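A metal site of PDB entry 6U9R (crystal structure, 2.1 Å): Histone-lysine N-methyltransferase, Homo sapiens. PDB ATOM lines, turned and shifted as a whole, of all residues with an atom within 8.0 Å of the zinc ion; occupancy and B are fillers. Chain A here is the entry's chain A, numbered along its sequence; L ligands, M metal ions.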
ATOM      1  N   ILE A  27      -3.385 -14.907   8.217  1.00  0.00           N
ATOM      2  CA  ILE A  27      -4.346 -15.493   9.142  1.00  0.00           C
ATOM      3  C   ILE A  27      -3.905 -15.084  10.551  1.00  0.00           C
ATOM      4  O   ILE A  27      -4.668 -14.426  11.241  1.00  0.00           O
ATOM      5  CB  ILE A  27      -4.526 -17.045   8.957  1.00  0.00           C
ATOM      6  CG1 ILE A  27      -5.254 -17.361   7.646  1.00  0.00           C
ATOM      7  CG2 ILE A  27      -5.264 -17.654  10.138  1.00  0.00           C
ATOM      8  CD1 ILE A  27      -5.080 -18.861   7.141  1.00  0.00           C
ATOM      9  N   HIS A  96      -5.153 -22.541  11.929  1.00  0.00           N
ATOM     10  CA  HIS A  96      -6.504 -23.082  11.813  1.00  0.00           C
ATOM     11  C   HIS A  96      -7.253 -22.485  10.607  1.00  0.00           C
ATOM     12  O   HIS A  96      -6.999 -21.335  10.239  1.00  0.00           O
ATOM     13  CB  HIS A  96      -7.296 -22.751  13.105  1.00  0.00           C
ATOM     14  CG  HIS A  96      -8.763 -23.017  12.983  1.00  0.00           C
ATOM     15  ND1 HIS A  96      -9.271 -24.297  12.997  1.00  0.00           N
ATOM     16  CD2 HIS A  96      -9.778 -22.145  12.795  1.00  0.00           C
ATOM     17  CE1 HIS A  96     -10.578 -24.160  12.825  1.00  0.00           C
ATOM     18  NE2 HIS A  96     -10.920 -22.881  12.682  1.00  0.00           N
ATOM     19  N   SER A  97      -8.191 -23.264  10.023  1.00  0.00           N
ATOM     20  CA  SER A  97      -9.099 -22.814   8.954  1.00  0.00           C
ATOM     21  C   SER A  97     -10.364 -23.633   8.948  1.00  0.00           C
ATOM     22  O   SER A  97     -10.311 -24.826   9.210  1.00  0.00           O
ATOM     23  CB  SER A  97      -8.436 -22.862   7.579  1.00  0.00           C
ATOM     24  OG  SER A  97      -9.344 -22.547   6.533  1.00  0.00           O
ATOM     25  N   CYS A  98     -11.481 -22.989   8.587  1.00  0.00           N
ATOM     26  CA  CYS A  98     -12.824 -23.584   8.528  1.00  0.00           C
ATOM     27  C   CYS A  98     -13.090 -24.242   7.174  1.00  0.00           C
ATOM     28  O   CYS A  98     -14.102 -24.935   7.005  1.00  0.00           O
ATOM     29  CB  CYS A  98     -13.881 -22.553   8.897  1.00  0.00           C
ATOM     30  SG  CYS A  98     -13.512 -21.666  10.425  1.00  0.00           S
ATOM     31  N   GLU A  99     -12.161 -24.027   6.234  1.00  0.00           N
ATOM     32  CA  GLU A  99     -12.148 -24.668   4.921  1.00  0.00           C
ATOM     33  C   GLU A  99     -10.661 -25.083   4.779  1.00  0.00           C
ATOM     34  O   GLU A  99      -9.918 -24.461   4.023  1.00  0.00           O
ATOM     35  CB  GLU A  99     -12.601 -23.711   3.810  1.00  0.00           C
ATOM     36  N   ASP A 132      -8.447 -27.996  10.537  1.00  0.00           N
ATOM     37  CA  ASP A 132      -9.499 -27.608  11.467  1.00  0.00           C
ATOM     38  C   ASP A 132      -8.999 -28.009  12.840  1.00  0.00           C
ATOM     39  O   ASP A 132      -8.734 -29.200  13.081  1.00  0.00           O
ATOM     40  CB  ASP A 132     -10.822 -28.350  11.140  1.00  0.00           C
ATOM     41  CG  ASP A 132     -12.067 -27.729  11.749  1.00  0.00           C
ATOM     42  OD1 ASP A 132     -12.092 -27.507  12.989  1.00  0.00           O
ATOM     43  OD2 ASP A 132     -13.049 -27.493  10.993  1.00  0.00           O
ATOM     44  N   PRO A 145     -11.731 -15.537  18.270  1.00  0.00           N
ATOM     45  CA  PRO A 145     -12.127 -15.281  16.866  1.00  0.00           C
ATOM     46  C   PRO A 145     -11.237 -15.908  15.810  1.00  0.00           C
ATOM     47  O   PRO A 145     -10.032 -16.055  16.026  1.00  0.00           O
ATOM     48  CB  PRO A 145     -12.152 -13.749  16.766  1.00  0.00           C
ATOM     49  CG  PRO A 145     -11.236 -13.282  17.837  1.00  0.00           C
ATOM     50  CD  PRO A 145     -11.276 -14.298  18.944  1.00  0.00           C
ATOM     51  N   CYS A 146     -11.831 -16.294  14.655  1.00  0.00           N
ATOM     52  CA  CYS A 146     -11.133 -16.930  13.544  1.00  0.00           C
ATOM     53  C   CYS A 146     -10.941 -16.004  12.338  1.00  0.00           C
ATOM     54  O   CYS A 146     -11.897 -15.343  11.899  1.00  0.00           O
ATOM     55  CB  CYS A 146     -11.830 -18.231  13.157  1.00  0.00           C
ATOM     56  SG  CYS A 146     -11.307 -18.899  11.562  1.00  0.00           S
ATOM     57  N   ASN A 147      -9.713 -16.007  11.784  1.00  0.00           N
ATOM     58  CA  ASN A 147      -9.298 -15.177  10.659  1.00  0.00           C
ATOM     59  C   ASN A 147      -8.960 -15.972   9.379  1.00  0.00           C
ATOM     60  O   ASN A 147      -8.279 -15.442   8.487  1.00  0.00           O
ATOM     61  CB  ASN A 147      -8.122 -14.272  11.094  1.00  0.00           C
ATOM     62  CG  ASN A 147      -7.913 -13.041  10.247  1.00  0.00           C
ATOM     63  OD1 ASN A 147      -8.844 -12.268   9.973  1.00  0.00           O
ATOM     64  ND2 ASN A 147      -6.692 -12.812   9.813  1.00  0.00           N
ATOM     65  N   CYS A 148      -9.464 -17.219   9.248  1.00  0.00           N
ATOM     66  CA  CYS A 148      -9.158 -18.029   8.062  1.00  0.00           C
ATOM     67  C   CYS A 148      -9.593 -17.353   6.751  1.00  0.00           C
ATOM     68  O   CYS A 148      -8.945 -17.550   5.721  1.00  0.00           O
ATOM     69  CB  CYS A 148      -9.729 -19.436   8.172  1.00  0.00           C
ATOM     70  SG  CYS A 148     -11.512 -19.550   7.879  1.00  0.00           S
ATOM     71  N   GLY A 149     -10.704 -16.605   6.834  1.00  0.00           N
ATOM     72  CA  GLY A 149     -11.287 -15.816   5.754  1.00  0.00           C
ATOM     73  C   GLY A 149     -12.177 -16.570   4.783  1.00  0.00           C
ATOM     74  O   GLY A 149     -12.637 -15.956   3.824  1.00  0.00           O
ATOM     75  N   ALA A 150     -12.431 -17.872   5.021  1.00  0.00           N
ATOM     76  CA  ALA A 150     -13.264 -18.706   4.140  1.00  0.00           C
ATOM     77  C   ALA A 150     -14.720 -18.223   4.096  1.00  0.00           C
ATOM     78  O   ALA A 150     -15.171 -17.586   5.055  1.00  0.00           O
ATOM     79  CB  ALA A 150     -13.210 -20.160   4.586  1.00  0.00           C
ATOM     80  N   LYS A 151     -15.440 -18.481   2.986  1.00  0.00           N
ATOM     81  CA  LYS A 151     -16.857 -18.064   2.857  1.00  0.00           C
ATOM     82  C   LYS A 151     -17.689 -18.668   4.025  1.00  0.00           C
ATOM     83  O   LYS A 151     -18.362 -17.939   4.746  1.00  0.00           O
ATOM     84  CB  LYS A 151     -17.440 -18.470   1.483  1.00  0.00           C
ATOM     85  CG  LYS A 151     -18.909 -18.103   1.266  1.00  0.00           C
ATOM     86  N   LYS A 152     -17.559 -19.990   4.217  1.00  0.00           N
ATOM     87  CA  LYS A 152     -18.245 -20.784   5.230  1.00  0.00           C
ATOM     88  C   LYS A 152     -17.479 -20.819   6.580  1.00  0.00           C
ATOM     89  O   LYS A 152     -17.361 -21.869   7.215  1.00  0.00           O
ATOM     90  CB  LYS A 152     -18.479 -22.210   4.674  1.00  0.00           C
ATOM     91  N   CYS A 153     -16.972 -19.654   7.016  1.00  0.00           N
ATOM     92  CA  CYS A 153     -16.211 -19.517   8.262  1.00  0.00           C
ATOM     93  C   CYS A 153     -17.103 -19.721   9.494  1.00  0.00           C
ATOM     94  O   CYS A 153     -18.166 -19.121   9.573  1.00  0.00           O
ATOM     95  CB  CYS A 153     -15.495 -18.172   8.309  1.00  0.00           C
ATOM     96  SG  CYS A 153     -14.417 -17.955   9.753  1.00  0.00           S
ATOM     97  N   ARG A 154     -16.643 -20.540  10.473  1.00  0.00           N
ATOM     98  CA  ARG A 154     -17.360 -20.800  11.745  1.00  0.00           C
ATOM     99  C   ARG A 154     -17.247 -19.579  12.670  1.00  0.00           C
ATOM    100  O   ARG A 154     -17.945 -19.503  13.680  1.00  0.00           O
ATOM    101  CB  ARG A 154     -16.831 -22.065  12.439  1.00  0.00           C
ATOM    102  N   LYS A 155     -16.349 -18.622  12.300  1.00  0.00           N
ATOM    103  CA  LYS A 155     -16.049 -17.318  12.897  1.00  0.00           C
ATOM    104  C   LYS A 155     -15.368 -17.375  14.281  1.00  0.00           C
ATOM    105  O   LYS A 155     -14.920 -16.332  14.790  1.00  0.00           O
ATOM    106  CB  LYS A 155     -17.285 -16.418  12.913  1.00  0.00           C
ATOM    107  CG  LYS A 155     -17.912 -16.218  11.509  1.00  0.00           C
ATOM    108  CD  LYS A 155     -17.085 -15.299  10.587  1.00  0.00           C
ATOM    109  CE  LYS A 155     -17.798 -14.983   9.294  1.00  0.00           C
ATOM    110  NZ  LYS A 155     -16.996 -14.079   8.430  1.00  0.00           N
ATOM    111  N   PHE A 156     -15.209 -18.603  14.857  1.00  0.00           N
ATOM    112  CA  PHE A 156     -14.512 -18.853  16.126  1.00  0.00           C
ATOM    113  C   PHE A 156     -13.715 -20.149  16.065  1.00  0.00           C
ATOM    114  O   PHE A 156     -14.116 -21.107  15.391  1.00  0.00           O
ATOM    115  CB  PHE A 156     -15.465 -18.804  17.335  1.00  0.00           C
ATOM    116  CG  PHE A 156     -16.062 -17.442  17.609  1.00  0.00           C
ATOM    117  CD1 PHE A 156     -15.349 -16.479  18.311  1.00  0.00           C
ATOM    118  CD2 PHE A 156     -17.315 -17.109  17.093  1.00  0.00           C
ATOM    119  CE1 PHE A 156     -15.895 -15.201  18.510  1.00  0.00           C
ATOM    120  CE2 PHE A 156     -17.843 -15.820  17.285  1.00  0.00           C
ATOM    121  CZ  PHE A 156     -17.131 -14.883  17.998  1.00  0.00           C
ATOM    122  N   LEU A 157     -12.541 -20.170  16.741  1.00  0.00           N
ATOM    123  CA  LEU A 157     -11.666 -21.347  16.790  1.00  0.00           C
ATOM    124  C   LEU A 157     -12.168 -22.363  17.811  1.00  0.00           C
ATOM    125  O   LEU A 157     -13.033 -22.041  18.627  1.00  0.00           O
ATOM    126  CB  LEU A 157     -10.215 -20.940  17.106  1.00  0.00           C
HETATM  127  C1  LIG L   1      -7.075 -16.598  14.378  1.00  0.00           C
HETATM  128  O1  LIG L   1      -4.064 -20.693  19.324  1.00  0.00           O
HETATM  129  O2  LIG L   1       2.810 -17.608  14.642  1.00  0.00           O
HETATM  130  C2  LIG L   1      -5.477 -18.189  14.709  1.00  0.00           C
HETATM  131  N1  LIG L   1      -7.712 -19.173  11.965  1.00  0.00           N
HETATM  132  C3  LIG L   1      -5.994 -18.988  13.652  1.00  0.00           C
HETATM  133  O3  LIG L   1       3.150 -19.043  16.261  1.00  0.00           O
HETATM  134  C4  LIG L   1      -4.264 -20.081  14.372  1.00  0.00           C
HETATM  135  C5  LIG L   1      -3.638 -18.547  16.399  1.00  0.00           C
HETATM  136  C6  LIG L   1      -4.456 -18.953  17.681  1.00  0.00           C
HETATM  137  C7  LIG L   1      -3.936 -20.347  17.984  1.00  0.00           C
HETATM  138  C8  LIG L   1      -2.451 -20.158  17.541  1.00  0.00           C
HETATM  139  C9  LIG L   1      -1.799 -21.492  17.115  1.00  0.00           C
HETATM  140  C10 LIG L   1       0.617 -21.711  17.717  1.00  0.00           C
HETATM  141  C11 LIG L   1       0.457 -20.841  18.983  1.00  0.00           C
HETATM  142  C12 LIG L   1       1.599 -20.873  20.026  1.00  0.00           C
HETATM  143  C13 LIG L   1       2.882 -18.606  20.009  1.00  0.00           C
HETATM  144  C14 LIG L   1       2.456 -17.162  19.797  1.00  0.00           C
HETATM  145  C15 LIG L   1       2.765 -16.498  18.594  1.00  0.00           C
HETATM  146  C16 LIG L   1       2.281 -15.178  18.413  1.00  0.00           C
HETATM  147  C17 LIG L   1       1.536 -14.491  19.364  1.00  0.00           C
HETATM  148  C18 LIG L   1       1.245 -15.158  20.580  1.00  0.00           C
HETATM  149  C19 LIG L   1       2.416 -18.644  15.376  1.00  0.00           C
HETATM  150  C20 LIG L   1       1.027 -19.193  15.012  1.00  0.00           C
HETATM  151  N2  LIG L   1       0.474 -18.580  13.782  1.00  0.00           N
HETATM  152  C21 LIG L   1       1.186 -20.720  14.778  1.00  0.00           C
HETATM  153  C22 LIG L   1      -0.067 -21.511  15.256  1.00  0.00           C
HETATM  154  N3  LIG L   1      -0.360 -21.212  16.726  1.00  0.00           N
HETATM  155  O4  LIG L   1      -4.012 -18.103  18.672  1.00  0.00           O
HETATM  156  O5  LIG L   1      -2.464 -19.288  16.412  1.00  0.00           O
HETATM  157  N4  LIG L   1      -4.375 -18.914  15.189  1.00  0.00           N
HETATM  158  N5  LIG L   1      -5.980 -16.952  15.113  1.00  0.00           N
HETATM  159  N6  LIG L   1      -7.686 -17.281  13.354  1.00  0.00           N
HETATM  160  N7  LIG L   1      -5.220 -20.151  13.448  1.00  0.00           N
HETATM  161  C23 LIG L   1      -7.147 -18.482  12.987  1.00  0.00           C
HETATM  162  C24 LIG L   1       0.805 -19.326  18.788  1.00  0.00           C
HETATM  163  N8  LIG L   1       1.602 -19.357  20.036  1.00  0.00           N
HETATM  164  C25 LIG L   1       1.702 -16.501  20.796  1.00  0.00           C
HETATM  165 CL1  LIG L   1       2.685 -14.359  16.957  1.00  0.00          CL
HETATM  166 ZN    ZN M   1     -12.607 -19.669   9.852  1.00  0.00          ZN
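SG of Cys 153 sits close to N of Lys 155, at 3.3 Å.
The side-chain sulfur (SG) of Cys 148 lies close to the backbone NH (N) of Ala 150 (3.4 Å).
N of Cys 146 sits at hydrogen-bond distance from O of Lys 155 (3.1 Å).
NE2 of His 96 lies close to SG of Cys 98 (3.6 Å).
N of Arg 154 lies close to SG of Cys 98, at 3.3 Å.
N of His 96 sits at hydrogen-bond distance from N7 of the ligand, 2.8 Å away.
A nitrogen (N1) of the ligand lies within hydrogen-bond range of the backbone carbonyl oxygen (O) of His 96 (2.9 Å).
N of Asn 147 is in hydrogen-bond range of N6 of the ligand, 2.9 Å away.
The side-chain sulfur of Cys 146 sits close to a nitrogen (N1) of the ligand (3.6 Å).
The zinc ion is bound by the side-chain sulfur of Cys 148 (2.3 Å), the side-chain sulfur of Cys 98 (2.3 Å), the side-chain sulfur of Cys 146 (2.3 Å) and the side-chain sulfur of Cys 153 (2.5 Å).
Within 4 Å of the zinc ion: Cys 98, Cys 146, Cys 148 and Cys 153.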
